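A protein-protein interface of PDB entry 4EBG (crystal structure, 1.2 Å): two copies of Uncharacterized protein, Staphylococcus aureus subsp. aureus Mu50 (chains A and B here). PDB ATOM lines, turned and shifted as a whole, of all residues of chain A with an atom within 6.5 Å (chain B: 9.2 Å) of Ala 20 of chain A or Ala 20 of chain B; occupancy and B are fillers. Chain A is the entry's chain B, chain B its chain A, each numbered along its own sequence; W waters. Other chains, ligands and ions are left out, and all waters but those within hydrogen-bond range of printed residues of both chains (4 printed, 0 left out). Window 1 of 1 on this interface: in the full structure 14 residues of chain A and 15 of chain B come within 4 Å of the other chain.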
ATOM      1  N   GLN A  15     -16.384 -21.587 -10.549  1.00  0.00           N
ATOM      2  CA  GLN A  15     -17.633 -22.236 -10.182  1.00  0.00           C
ATOM      3  C   GLN A  15     -18.768 -21.610 -10.949  1.00  0.00           C
ATOM      4  O   GLN A  15     -19.629 -22.307 -11.510  1.00  0.00           O
ATOM      5  CB  GLN A  15     -17.872 -22.145  -8.674  1.00  0.00           C
ATOM      6  CG  GLN A  15     -17.014 -23.108  -7.853  1.00  0.00           C
ATOM      7  CD  GLN A  15     -17.185 -22.922  -6.367  1.00  0.00           C
ATOM      8  OE1 GLN A  15     -17.359 -21.808  -5.890  1.00  0.00           O
ATOM      9  NE2 GLN A  15     -17.118 -24.009  -5.627  1.00  0.00           N
ATOM     10  N   MET A  16     -18.843 -20.281 -10.961  1.00  0.00           N
ATOM     11  CA  MET A  16     -19.908 -19.618 -11.713  1.00  0.00           C
ATOM     12  C   MET A  16     -19.802 -19.850 -13.207  1.00  0.00           C
ATOM     13  O   MET A  16     -20.777 -20.079 -13.871  1.00  0.00           O
ATOM     14  CB  MET A  16     -19.900 -18.119 -11.412  1.00  0.00           C
ATOM     15  CG  MET A  16     -20.313 -17.805  -9.965  1.00  0.00           C
ATOM     16  SD  MET A  16     -20.564 -15.933  -9.661  1.00  0.00           S
ATOM     17  CE  MET A  16     -18.790 -15.475  -9.991  1.00  0.00           C
ATOM     18  N   ASN A  17     -18.569 -19.832 -13.733  1.00  0.00           N
ATOM     19  CA  ASN A  17     -18.415 -20.039 -15.181  1.00  0.00           C
ATOM     20  C   ASN A  17     -18.832 -21.456 -15.556  1.00  0.00           C
ATOM     21  O   ASN A  17     -19.363 -21.646 -16.634  1.00  0.00           O
ATOM     22  CB  ASN A  17     -16.975 -19.806 -15.662  1.00  0.00           C
ATOM     23  CG  ASN A  17     -16.591 -18.352 -15.753  1.00  0.00           C
ATOM     24  OD1 ASN A  17     -17.247 -17.453 -15.220  1.00  0.00           O
ATOM     25  ND2 ASN A  17     -15.488 -18.112 -16.470  1.00  0.00           N
ATOM     26  N   LYS A  18     -18.583 -22.420 -14.675  1.00  0.00           N
ATOM     27  CA  LYS A  18     -18.957 -23.805 -14.967  1.00  0.00           C
ATOM     28  C   LYS A  18     -20.474 -23.906 -15.112  1.00  0.00           C
ATOM     29  O   LYS A  18     -20.979 -24.546 -16.028  1.00  0.00           O
ATOM     30  CB  LYS A  18     -18.481 -24.768 -13.890  1.00  0.00           C
ATOM     31  CG  LYS A  18     -18.984 -26.195 -14.107  1.00  0.00           C
ATOM     32  CD  LYS A  18     -18.927 -27.007 -12.827  1.00  0.00           C
ATOM     33  CE  LYS A  18     -20.233 -27.780 -12.597  1.00  0.00           C
ATOM     34  NZ  LYS A  18     -21.254 -27.045 -11.769  1.00  0.00           N
ATOM     35  N   ILE A  19     -21.218 -23.262 -14.219  1.00  0.00           N
ATOM     36  CA  ILE A  19     -22.681 -23.303 -14.278  1.00  0.00           C
ATOM     37  C   ILE A  19     -23.123 -22.534 -15.545  1.00  0.00           C
ATOM     38  O   ILE A  19     -23.994 -23.001 -16.312  1.00  0.00           O
ATOM     39  CB  ILE A  19     -23.296 -22.731 -12.962  1.00  0.00           C
ATOM     40  CG1 ILE A  19     -22.920 -23.606 -11.765  1.00  0.00           C
ATOM     41  CG2 ILE A  19     -24.808 -22.665 -13.067  1.00  0.00           C
ATOM     42  CD1 ILE A  19     -23.262 -23.016 -10.425  1.00  0.00           C
ATOM     43  N   ALA A  20     -22.549 -21.348 -15.746  1.00  0.00           N
ATOM     44  CA  ALA A  20     -22.881 -20.567 -16.923  1.00  0.00           C
ATOM     45  C   ALA A  20     -22.682 -21.334 -18.214  1.00  0.00           C
ATOM     46  O   ALA A  20     -23.470 -21.194 -19.144  1.00  0.00           O
ATOM     47  CB  ALA A  20     -22.104 -19.214 -16.902  1.00  0.00           C
ATOM     48  N   SER A  21     -21.617 -22.119 -18.299  1.00  0.00           N
ATOM     49  CA  SER A  21     -21.280 -22.864 -19.492  1.00  0.00           C
ATOM     50  C   SER A  21     -22.347 -23.894 -19.866  1.00  0.00           C
ATOM     51  O   SER A  21     -22.383 -24.322 -20.994  1.00  0.00           O
ATOM     52  CB  SER A  21     -19.906 -23.543 -19.344  1.00  0.00           C
ATOM     53  OG  SER A  21     -19.978 -24.682 -18.481  1.00  0.00           O
ATOM     54  N   LYS A  22     -23.173 -24.312 -18.911  1.00  0.00           N
ATOM     55  CA  LYS A  22     -24.282 -25.246 -19.171  1.00  0.00           C
ATOM     56  C   LYS A  22     -25.336 -24.600 -20.037  1.00  0.00           C
ATOM     57  O   LYS A  22     -26.015 -25.271 -20.840  1.00  0.00           O
ATOM     58  CB  LYS A  22     -24.891 -25.779 -17.864  1.00  0.00           C
ATOM     59  CG  LYS A  22     -23.871 -26.544 -16.960  1.00  0.00           C
ATOM     60  CD  LYS A  22     -24.420 -27.008 -15.568  1.00  0.00           C
ATOM     61  CE  LYS A  22     -23.344 -27.704 -14.703  1.00  0.00           C
ATOM     62  NZ  LYS A  22     -23.742 -27.697 -13.258  1.00  0.00           N
ATOM     63  N   VAL A  23     -25.495 -23.295 -19.883  1.00  0.00           N
ATOM     64  CA  VAL A  23     -26.488 -22.616 -20.687  1.00  0.00           C
ATOM     65  C   VAL A  23     -25.906 -21.779 -21.819  1.00  0.00           C
ATOM     66  O   VAL A  23     -26.591 -21.471 -22.775  1.00  0.00           O
ATOM     67  CB  VAL A  23     -27.502 -21.821 -19.831  1.00  0.00           C
ATOM     68  CG1 VAL A  23     -28.175 -22.739 -18.772  1.00  0.00           C
ATOM     69  CG2 VAL A  23     -26.815 -20.649 -19.185  1.00  0.00           C
ATOM     70  N   GLN A  24     -24.602 -21.462 -21.739  1.00  0.00           N
ATOM     71  CA  GLN A  24     -23.925 -20.730 -22.815  1.00  0.00           C
ATOM     72  C   GLN A  24     -22.539 -21.329 -22.912  1.00  0.00           C
ATOM     73  O   GLN A  24     -21.599 -20.970 -22.233  1.00  0.00           O
ATOM     74  CB  GLN A  24     -23.898 -19.198 -22.621  1.00  0.00           C
ATOM     75  CG  GLN A  24     -23.070 -18.416 -23.667  1.00  0.00           C
ATOM     76  CD  GLN A  24     -23.183 -16.895 -23.488  1.00  0.00           C
ATOM     77  OE1 GLN A  24     -23.675 -16.420 -22.458  1.00  0.00           O
ATOM     78  NE2 GLN A  24     -22.736 -16.144 -24.479  1.00  0.00           N
ATOM     79  N   ASN A  25     -22.401 -22.280 -23.842  1.00  0.00           N
ATOM     80  CA  ASN A  25     -21.245 -23.174 -23.847  1.00  0.00           C
ATOM     81  C   ASN A  25     -19.946 -22.596 -24.401  1.00  0.00           C
ATOM     82  O   ASN A  25     -18.937 -23.287 -24.438  1.00  0.00           O
ATOM     83  CB  ASN A  25     -21.592 -24.534 -24.476  1.00  0.00           C
ATOM     84  CG  ASN A  25     -21.856 -24.453 -25.955  1.00  0.00           C
ATOM     85  OD1 ASN A  25     -21.632 -23.430 -26.591  1.00  0.00           O
ATOM     86  ND2 ASN A  25     -22.333 -25.575 -26.529  1.00  0.00           N
ATOM     87  N   ILE A  27     -18.519 -20.148 -22.794  1.00  0.00           N
ATOM     88  CA  ILE A  27     -17.859 -19.690 -21.570  1.00  0.00           C
ATOM     89  C   ILE A  27     -16.735 -20.631 -21.150  1.00  0.00           C
ATOM     90  O   ILE A  27     -16.901 -21.831 -21.095  1.00  0.00           O
ATOM     91  CB  ILE A  27     -18.899 -19.458 -20.417  1.00  0.00           C
ATOM     92  CG1 ILE A  27     -19.786 -18.266 -20.777  1.00  0.00           C
ATOM     93  CG2 ILE A  27     -18.235 -19.225 -19.065  1.00  0.00           C
ATOM     94  CD1 ILE A  27     -20.934 -18.006 -19.827  1.00  0.00           C
ATOM     95  N   ARG A  76     -21.598  -7.040  -9.218  1.00  0.00           N
ATOM     96  CA  ARG A  76     -21.781  -6.431 -10.516  1.00  0.00           C
ATOM     97  C   ARG A  76     -22.271  -4.979 -10.423  1.00  0.00           C
ATOM     98  O   ARG A  76     -22.304  -4.333 -11.445  1.00  0.00           O
ATOM     99  CB  ARG A  76     -22.713  -7.281 -11.397  1.00  0.00           C
ATOM    100  CG  ARG A  76     -22.137  -8.675 -11.785  1.00  0.00           C
ATOM    101  CD  ARG A  76     -20.770  -8.634 -12.398  1.00  0.00           C
ATOM    102  NE  ARG A  76     -20.698  -7.770 -13.570  1.00  0.00           N
ATOM    103  CZ  ARG A  76     -21.106  -8.064 -14.798  1.00  0.00           C
ATOM    104  NH1 ARG A  76     -21.600  -9.246 -15.098  1.00  0.00           N
ATOM    105  NH2 ARG A  76     -20.985  -7.169 -15.765  1.00  0.00           N
ATOM    106  N   GLU B  12     -34.936 -25.201 -12.393  1.00  0.00           N
ATOM    107  CA  GLU B  12     -33.520 -25.464 -12.642  1.00  0.00           C
ATOM    108  C   GLU B  12     -32.929 -24.527 -13.681  1.00  0.00           C
ATOM    109  O   GLU B  12     -31.845 -23.996 -13.487  1.00  0.00           O
ATOM    110  CB  GLU B  12     -33.326 -26.921 -13.055  1.00  0.00           C
ATOM    111  CG  GLU B  12     -31.893 -27.337 -13.255  1.00  0.00           C
ATOM    112  CD  GLU B  12     -31.035 -27.349 -12.073  1.00  0.00           C
ATOM    113  OE1 GLU B  12     -31.542 -27.335 -10.931  1.00  0.00           O
ATOM    114  OE2 GLU B  12     -29.815 -27.394 -12.330  1.00  0.00           O
ATOM    115  N   GLN B  13     -33.643 -24.304 -14.770  1.00  0.00           N
ATOM    116  CA  GLN B  13     -33.146 -23.388 -15.795  1.00  0.00           C
ATOM    117  C   GLN B  13     -32.954 -22.009 -15.188  1.00  0.00           C
ATOM    118  O   GLN B  13     -31.941 -21.347 -15.443  1.00  0.00           O
ATOM    119  CB  GLN B  13     -34.132 -23.285 -16.960  1.00  0.00           C
ATOM    120  CG  GLN B  13     -33.657 -22.403 -18.038  1.00  0.00           C
ATOM    121  CD  GLN B  13     -32.586 -23.024 -18.886  1.00  0.00           C
ATOM    122  OE1 GLN B  13     -32.729 -24.151 -19.339  1.00  0.00           O
ATOM    123  NE2 GLN B  13     -31.475 -22.284 -19.135  1.00  0.00           N
ATOM    124  N   ASN B  14     -33.909 -21.554 -14.396  1.00  0.00           N
ATOM    125  CA  ASN B  14     -33.810 -20.234 -13.768  1.00  0.00           C
ATOM    126  C   ASN B  14     -32.704 -20.105 -12.770  1.00  0.00           C
ATOM    127  O   ASN B  14     -32.056 -19.083 -12.711  1.00  0.00           O
ATOM    128  CB  ASN B  14     -35.139 -19.782 -13.213  1.00  0.00           C
ATOM    129  CG  ASN B  14     -36.029 -19.287 -14.312  1.00  0.00           C
ATOM    130  OD1 ASN B  14     -35.569 -18.521 -15.143  1.00  0.00           O
ATOM    131  ND2 ASN B  14     -37.290 -19.701 -14.334  1.00  0.00           N
ATOM    132  N   GLN B  15     -32.441 -21.164 -12.022  1.00  0.00           N
ATOM    133  CA  GLN B  15     -31.322 -21.173 -11.065  1.00  0.00           C
ATOM    134  C   GLN B  15     -29.998 -21.021 -11.808  1.00  0.00           C
ATOM    135  O   GLN B  15     -29.109 -20.221 -11.429  1.00  0.00           O
ATOM    136  CB  GLN B  15     -31.336 -22.475 -10.272  1.00  0.00           C
ATOM    137  CG  GLN B  15     -32.363 -22.474  -9.162  1.00  0.00           C
ATOM    138  CD  GLN B  15     -32.351 -23.745  -8.336  1.00  0.00           C
ATOM    139  OE1 GLN B  15     -31.501 -24.624  -8.518  1.00  0.00           O
ATOM    140  NE2 GLN B  15     -33.285 -23.841  -7.410  1.00  0.00           N
ATOM    141  N   MET B  16     -29.833 -21.763 -12.901  1.00  0.00           N
ATOM    142  CA  MET B  16     -28.603 -21.660 -13.710  1.00  0.00           C
ATOM    143  C   MET B  16     -28.500 -20.298 -14.375  1.00  0.00           C
ATOM    144  O   MET B  16     -27.441 -19.726 -14.450  1.00  0.00           O
ATOM    145  CB  MET B  16     -28.532 -22.776 -14.755  1.00  0.00           C
ATOM    146  CG  MET B  16     -28.382 -24.154 -14.098  1.00  0.00           C
ATOM    147  SD  MET B  16     -28.023 -25.515 -15.393  1.00  0.00           S
ATOM    148  CE  MET B  16     -29.789 -25.442 -16.192  1.00  0.00           C
ATOM    149  N   ASN B  17     -29.616 -19.812 -14.902  1.00  0.00           N
ATOM    150  CA  ASN B  17     -29.570 -18.490 -15.582  1.00  0.00           C
ATOM    151  C   ASN B  17     -29.236 -17.367 -14.618  1.00  0.00           C
ATOM    152  O   ASN B  17     -28.521 -16.436 -14.983  1.00  0.00           O
ATOM    153  CB  ASN B  17     -30.887 -18.152 -16.281  1.00  0.00           C
ATOM    154  CG  ASN B  17     -31.081 -18.873 -17.598  1.00  0.00           C
ATOM    155  OD1 ASN B  17     -30.493 -19.908 -17.832  1.00  0.00           O
ATOM    156  ND2 ASN B  17     -31.904 -18.318 -18.474  1.00  0.00           N
ATOM    157  N   LYS B  18     -29.706 -17.472 -13.402  1.00  0.00           N
ATOM    158  CA  LYS B  18     -29.390 -16.470 -12.394  1.00  0.00           C
ATOM    159  C   LYS B  18     -27.881 -16.386 -12.158  1.00  0.00           C
ATOM    160  O   LYS B  18     -27.320 -15.291 -12.066  1.00  0.00           O
ATOM    161  CB  LYS B  18     -30.081 -16.799 -11.079  1.00  0.00           C
ATOM    162  CG  LYS B  18     -30.050 -15.639 -10.076  1.00  0.00           C
ATOM    163  CD  LYS B  18     -30.934 -14.464 -10.578  1.00  0.00           C
ATOM    164  CE  LYS B  18     -30.646 -13.125  -9.883  1.00  0.00           C
ATOM    165  NZ  LYS B  18     -30.996 -11.970 -10.773  1.00  0.00           N
ATOM    166  N   ILE B  19     -27.249 -17.533 -11.993  1.00  0.00           N
ATOM    167  CA  ILE B  19     -25.817 -17.529 -11.784  1.00  0.00           C
ATOM    168  C   ILE B  19     -25.110 -17.069 -13.058  1.00  0.00           C
ATOM    169  O   ILE B  19     -24.173 -16.274 -13.002  1.00  0.00           O
ATOM    170  CB  ILE B  19     -25.356 -18.932 -11.284  1.00  0.00           C
ATOM    171  CG1 ILE B  19     -26.021 -19.273  -9.946  1.00  0.00           C
ATOM    172  CG2 ILE B  19     -23.843 -18.957 -11.111  1.00  0.00           C
ATOM    173  CD1 ILE B  19     -25.863 -20.752  -9.537  1.00  0.00           C
ATOM    174  N   ALA B  20     -25.508 -17.590 -14.210  1.00  0.00           N
ATOM    175  CA  ALA B  20     -24.919 -17.225 -15.471  1.00  0.00           C
ATOM    176  C   ALA B  20     -24.951 -15.723 -15.690  1.00  0.00           C
ATOM    177  O   ALA B  20     -23.970 -15.163 -16.202  1.00  0.00           O
ATOM    178  CB  ALA B  20     -25.577 -17.984 -16.642  1.00  0.00           C
ATOM    179  N   SER B  21     -26.040 -15.085 -15.298  1.00  0.00           N
ATOM    180  CA  SER B  21     -26.233 -13.646 -15.512  1.00  0.00           C
ATOM    181  C   SER B  21     -25.233 -12.794 -14.723  1.00  0.00           C
ATOM    182  O   SER B  21     -25.013 -11.647 -15.053  1.00  0.00           O
ATOM    183  CB  SER B  21     -27.677 -13.248 -15.179  1.00  0.00           C
ATOM    184  OG  SER B  21     -27.883 -13.221 -13.788  1.00  0.00           O
ATOM    185  N   LYS B  22     -24.647 -13.377 -13.673  1.00  0.00           N
ATOM    186  CA  LYS B  22     -23.613 -12.689 -12.905  1.00  0.00           C
ATOM    187  C   LYS B  22     -22.338 -12.521 -13.699  1.00  0.00           C
ATOM    188  O   LYS B  22     -21.628 -11.542 -13.507  1.00  0.00           O
ATOM    189  CB  LYS B  22     -23.309 -13.422 -11.603  1.00  0.00           C
ATOM    190  CG  LYS B  22     -24.512 -13.549 -10.669  1.00  0.00           C
ATOM    191  CD  LYS B  22     -24.276 -14.589  -9.589  1.00  0.00           C
ATOM    192  CE  LYS B  22     -25.373 -14.565  -8.525  1.00  0.00           C
ATOM    193  NZ  LYS B  22     -25.392 -15.789  -7.685  1.00  0.00           N
ATOM    194  N   VAL B  23     -22.073 -13.453 -14.622  1.00  0.00           N
ATOM    195  CA  VAL B  23     -20.847 -13.371 -15.390  1.00  0.00           C
ATOM    196  C   VAL B  23     -21.103 -12.907 -16.802  1.00  0.00           C
ATOM    197  O   VAL B  23     -20.158 -12.480 -17.443  1.00  0.00           O
ATOM    198  CB  VAL B  23     -19.961 -14.653 -15.355  1.00  0.00           C
ATOM    199  CG1 VAL B  23     -19.543 -14.929 -13.961  1.00  0.00           C
ATOM    200  CG2 VAL B  23     -20.705 -15.845 -15.916  1.00  0.00           C
ATOM    201  N   GLN B  24     -22.332 -13.044 -17.317  1.00  0.00           N
ATOM    202  CA  GLN B  24     -22.667 -12.666 -18.645  1.00  0.00           C
ATOM    203  C   GLN B  24     -24.067 -12.042 -18.568  1.00  0.00           C
ATOM    204  O   GLN B  24     -25.095 -12.732 -18.653  1.00  0.00           O
ATOM    205  CB  GLN B  24     -22.578 -13.933 -19.490  1.00  0.00           C
ATOM    206  CG  GLN B  24     -22.380 -13.679 -20.903  1.00  0.00           C
ATOM    207  CD  GLN B  24     -23.538 -12.944 -21.479  1.00  0.00           C
ATOM    208  OE1 GLN B  24     -23.688 -11.736 -21.273  1.00  0.00           O
ATOM    209  NE2 GLN B  24     -24.407 -13.666 -22.163  1.00  0.00           N
ATOM    210  N   ASN B  25     -24.135 -10.727 -18.338  1.00  0.00           N
ATOM    211  CA  ASN B  25     -25.385 -10.114 -17.916  1.00  0.00           C
ATOM    212  C   ASN B  25     -26.417  -9.918 -18.972  1.00  0.00           C
ATOM    213  O   ASN B  25     -27.454  -9.340 -18.673  1.00  0.00           O
ATOM    214  CB  ASN B  25     -25.126  -8.802 -17.180  1.00  0.00           C
ATOM    215  CG  ASN B  25     -24.566  -7.716 -18.065  1.00  0.00           C
ATOM    216  OD1 ASN B  25     -24.544  -7.817 -19.284  1.00  0.00           O
ATOM    217  ND2 ASN B  25     -24.168  -6.610 -17.445  1.00  0.00           N
ATOM    218  N   THR B  26     -26.161 -10.383 -20.190  1.00  0.00           N
ATOM    219  CA  THR B  26     -27.231 -10.431 -21.197  1.00  0.00           C
ATOM    220  C   THR B  26     -28.112 -11.686 -21.044  1.00  0.00           C
ATOM    221  O   THR B  26     -29.158 -11.734 -21.671  1.00  0.00           O
ATOM    222  CB  THR B  26     -26.734 -10.356 -22.635  1.00  0.00           C
ATOM    223  OG1 THR B  26     -25.884 -11.464 -22.907  1.00  0.00           O
ATOM    224  CG2 THR B  26     -25.981  -9.062 -22.854  1.00  0.00           C
ATOM    225  N   ILE B  27     -27.726 -12.638 -20.191  1.00  0.00           N
ATOM    226  CA  ILE B  27     -28.561 -13.817 -19.924  1.00  0.00           C
ATOM    227  C   ILE B  27     -29.811 -13.399 -19.168  1.00  0.00           C
ATOM    228  O   ILE B  27     -29.741 -12.725 -18.123  1.00  0.00           O
ATOM    229  CB  ILE B  27     -27.805 -14.888 -19.098  1.00  0.00           C
ATOM    230  CG1 ILE B  27     -26.664 -15.509 -19.908  1.00  0.00           C
ATOM    231  CG2 ILE B  27     -28.773 -15.986 -18.607  1.00  0.00           C
ATOM    232  CD1 ILE B  27     -27.068 -15.945 -21.314  1.00  0.00           C
ATOM    233  N   LYS B  28     -30.968 -13.799 -19.678  1.00  0.00           N
ATOM    234  CA  LYS B  28     -32.236 -13.415 -19.118  1.00  0.00           C
ATOM    235  C   LYS B  28     -32.564 -14.284 -17.918  1.00  0.00           C
ATOM    236  O   LYS B  28     -32.364 -15.516 -17.939  1.00  0.00           O
ATOM    237  CB  LYS B  28     -33.310 -13.559 -20.194  1.00  0.00           C
ATOM    238  CG  LYS B  28     -34.668 -13.089 -19.784  1.00  0.00           C
ATOM    239  CD  LYS B  28     -35.606 -13.015 -20.991  1.00  0.00           C
ATOM    240  CE  LYS B  28     -37.006 -12.662 -20.521  1.00  0.00           C
ATOM    241  NZ  LYS B  28     -37.074 -11.250 -20.032  1.00  0.00           N
ATOM    242  N   THR B  29     -33.099 -13.662 -16.893  1.00  0.00           N
ATOM    243  CA  THR B  29     -33.470 -14.389 -15.694  1.00  0.00           C
ATOM    244  C   THR B  29     -34.996 -14.502 -15.543  1.00  0.00           C
ATOM    245  O   THR B  29     -35.757 -13.831 -16.236  1.00  0.00           O
ATOM    246  CB  THR B  29     -32.803 -13.765 -14.440  1.00  0.00           C
ATOM    247  OG1 THR B  29     -33.299 -12.442 -14.272  1.00  0.00           O
ATOM    248  CG2 THR B  29     -31.281 -13.733 -14.574  1.00  0.00           C
ATOM    249  N   LEU B  53     -33.267 -16.959 -24.147  1.00  0.00           N
ATOM    250  CA  LEU B  53     -32.069 -17.033 -23.295  1.00  0.00           C
ATOM    251  C   LEU B  53     -31.438 -15.666 -23.054  1.00  0.00           C
ATOM    252  O   LEU B  53     -30.883 -15.414 -21.989  1.00  0.00           O
ATOM    253  CB  LEU B  53     -31.058 -18.006 -23.882  1.00  0.00           C
ATOM    254  CG  LEU B  53     -29.701 -18.231 -23.192  1.00  0.00           C
ATOM    255  CD1 LEU B  53     -29.917 -18.740 -21.779  1.00  0.00           C
ATOM    256  CD2 LEU B  53     -28.815 -19.143 -23.994  1.00  0.00           C
ATOM    257  N   TYR B  54     -31.486 -14.814 -24.059  1.00  0.00           N
ATOM    258  CA  TYR B  54     -30.781 -13.534 -24.020  1.00  0.00           C
ATOM    259  C   TYR B  54     -31.755 -12.387 -24.022  1.00  0.00           C
ATOM    260  O   TYR B  54     -32.680 -12.371 -24.804  1.00  0.00           O
ATOM    261  CB  TYR B  54     -29.778 -13.415 -25.161  1.00  0.00           C
ATOM    262  CG  TYR B  54     -28.704 -14.460 -25.206  1.00  0.00           C
ATOM    263  CD1 TYR B  54     -27.652 -14.462 -24.299  1.00  0.00           C
ATOM    264  CD2 TYR B  54     -28.770 -15.501 -26.110  1.00  0.00           C
ATOM    265  CE1 TYR B  54     -26.667 -15.444 -24.345  1.00  0.00           C
ATOM    266  CE2 TYR B  54     -27.814 -16.471 -26.161  1.00  0.00           C
ATOM    267  CZ  TYR B  54     -26.766 -16.449 -25.278  1.00  0.00           C
ATOM    268  OH  TYR B  54     -25.861 -17.467 -25.372  1.00  0.00           O
ATOM    269  N   PHE B  63     -33.082 -26.381 -24.916  1.00  0.00           N
ATOM    270  CA  PHE B  63     -32.377 -27.150 -23.944  1.00  0.00           C
ATOM    271  C   PHE B  63     -33.161 -28.425 -23.607  1.00  0.00           C
ATOM    272  O   PHE B  63     -34.385 -28.376 -23.419  1.00  0.00           O
ATOM    273  CB  PHE B  63     -32.152 -26.396 -22.643  1.00  0.00           C
ATOM    274  CG  PHE B  63     -31.313 -25.183 -22.794  1.00  0.00           C
ATOM    275  CD1 PHE B  63     -29.942 -25.269 -22.903  1.00  0.00           C
ATOM    276  CD2 PHE B  63     -31.904 -23.955 -22.831  1.00  0.00           C
ATOM    277  CE1 PHE B  63     -29.179 -24.128 -23.032  1.00  0.00           C
ATOM    278  CE2 PHE B  63     -31.123 -22.783 -22.986  1.00  0.00           C
ATOM    279  CZ  PHE B  63     -29.759 -22.890 -23.066  1.00  0.00           C
ATOM    280  N   ILE B  74     -30.223 -30.952 -16.709  1.00  0.00           N
ATOM    281  CA  ILE B  74     -29.961 -30.540 -18.061  1.00  0.00           C
ATOM    282  C   ILE B  74     -28.991 -31.541 -18.672  1.00  0.00           C
ATOM    283  O   ILE B  74     -28.124 -32.059 -18.001  1.00  0.00           O
ATOM    284  CB  ILE B  74     -29.405 -29.097 -18.101  1.00  0.00           C
ATOM    285  CG1 ILE B  74     -29.515 -28.524 -19.496  1.00  0.00           C
ATOM    286  CG2 ILE B  74     -27.952 -29.000 -17.590  1.00  0.00           C
ATOM    287  CD1 ILE B  74     -29.301 -26.996 -19.624  1.00  0.00           C
ATOM    288  N   ARG B  76     -26.712 -31.393 -22.001  1.00  0.00           N
ATOM    289  CA  ARG B  76     -26.189 -30.720 -23.188  1.00  0.00           C
ATOM    290  C   ARG B  76     -25.654 -31.672 -24.271  1.00  0.00           C
ATOM    291  O   ARG B  76     -25.314 -31.243 -25.339  1.00  0.00           O
ATOM    292  CB  ARG B  76     -25.128 -29.662 -22.789  1.00  0.00           C
ATOM    293  CG  ARG B  76     -25.726 -28.468 -21.984  1.00  0.00           C
ATOM    294  CD  ARG B  76     -26.935 -27.780 -22.652  1.00  0.00           C
ATOM    295  NE  ARG B  76     -26.753 -27.389 -24.037  1.00  0.00           N
ATOM    296  CZ  ARG B  76     -26.103 -26.311 -24.455  1.00  0.00           C
ATOM    297  NH1 ARG B  76     -25.571 -25.445 -23.587  1.00  0.00           N
ATOM    298  NH2 ARG B  76     -26.026 -26.105 -25.773  1.00  0.00           N
HETATM  299  O   HOH W   1     -24.741 -23.233 -25.384  1.00  0.00           O
HETATM  300  O   HOH W   2     -21.729  -9.138 -18.134  1.00  0.00           O
HETATM  301  O   HOH W   3     -21.187  -6.615 -18.840  1.00  0.00           O
HETATM  302  O   HOH W   4     -25.038 -24.195 -27.807  1.00  0.00           O
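Printed residues of chain B that touch a printed residue of chain A: Gln 13, Met 16, Asn 17, Ile 19, Ala 20, Lys 22, Val 23, Gln 24, Asn 25, Ile 27, Leu 53, Tyr 54, Phe 63, Ile 74 and Arg 76.
Of the 13 printed residues of chain A, 9 touch a printed residue of chain B.
Among the printed residues, no Asp or Glu carboxylate lies within 4 Å of a Lys or Arg side-chain nitrogen of the other chain.
Ile 19 of chain B touches Met 16 of chain A.
Lys 22 of chain B touches Met 16 of chain A (CD to SD, 3.9 Å).
Ile 19 of chain B touches Ile 19 of chain A (CD1 to CD1, 3.6 Å).
Ala 20 of chain A touches Val 23 of chain B (CB to CG2, 3.8 Å).
Lys 22 of chain A touches Met 16 of chain B (CD to SD, 3.9 Å).
Val 23 of chain A touches Gln 13 of chain B.
Asn 17 of chain B touches Val 23 of chain A (OD1 to CG1, 3.8 Å).
Phe 63 of chain B touches Val 23 of chain A.
Water W2 lies within hydrogen-bond range of the backbone NH of Asn 25 of chain B (2.9 Å) and the guanidinium group of Arg 76 of chain A (3.0 Å).
Water W1 bridges the backbone NH of Asn 25 of chain A (3.0 Å) and the guanidinium group of Arg 76 of chain B (3.0 Å).
Water W4 lies within hydrogen-bond range of NH2 of Arg 76 of chain B and ND2 of Asn 25 of chain A.
Water W3 bridges NH2 of Arg 76 of chain A and ND2 of Asn 25 of chain B.
O of Leu 53 of chain B sits at hydrogen-bond distance from N of Lys 28 of chain B, 2.8 Å away.
The side-chain amide oxygen (OD1) of Asn 17 of chain B sits at hydrogen-bond distance from the side-chain amide nitrogen (NE2) of Gln 13 of chain B, 2.9 Å away.
OE1 of Gln 24 of chain B sits at hydrogen-bond distance from OG1 of Thr 26 of chain B (2.8 Å).
O of Asn 17 of chain B sits close to OG of Ser 21 of chain B, at 3.5 Å.
O of Lys 28 of chain B lies within hydrogen-bond range of ND2 of Asn 17 of chain B.
The guanidinium group of Arg 76 of chain B sits at hydrogen-bond distance from the backbone carbonyl oxygen of Lys 22 of chain A (2.8 Å).
NH1 of Arg 76 of chain A sits at hydrogen-bond distance from O of Lys 22 of chain B (2.8 Å).
The side-chain amide nitrogen (NE2) of Gln 24 of chain B lies within hydrogen-bond range of the side-chain amide oxygen (OE1) of Gln 24 of chain A (2.9 Å).
Of the printed residues of chain B, Asn 17 of chain A touches Val 23 (3.6 Å).
Ala 20 of chain A touches just these residues of chain B: Ala 20 and Val 23.
Of the printed residues of chain B, Asn 25 of chain A touches Arg 76.
Glu 12 of chain B touches none of the printed residues of chain A.
Of chain A, only Ala 20 (3.7 Å) and Val 23 (3.9 Å) come within 4 Å of Ala 20 of chain B.
Of the printed residues of chain A, Lys 22 of chain B touches Met 16 (3.9 Å) and Arg 76 (2.8 Å).
Of the printed residues of chain A, Gln 24 of chain B touches Gln 24 (2.9 Å).
Thr 29 of chain B touches none of the printed residues of chain A.
The nearest printed residue of chain B that does not touch Ala 20 of chain A is Met 16 of chain B (5.3 Å).
The nearest printed residue of chain A that does not touch Ala 20 of chain B is Ile 19 of chain A (5.2 Å).
Asn 17 of chain A touches Val 23 of chain B, and with the chains exchanged Val 23 of chain A touches Asn 17 of chain B.
Ile 19 of chain A touches its own counterpart, Ile 19 of chain B.
Ala 20 of chain A touches Val 23 of chain B, and with the chains exchanged Val 23 of chain A touches Ala 20 of chain B.
Gln 24 of chain A touches its own counterpart, Gln 24 of chain B.
Of the 21 pairs that touch across the chains among the printed residues, 15 have their exchanged pair printed and touching as well.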
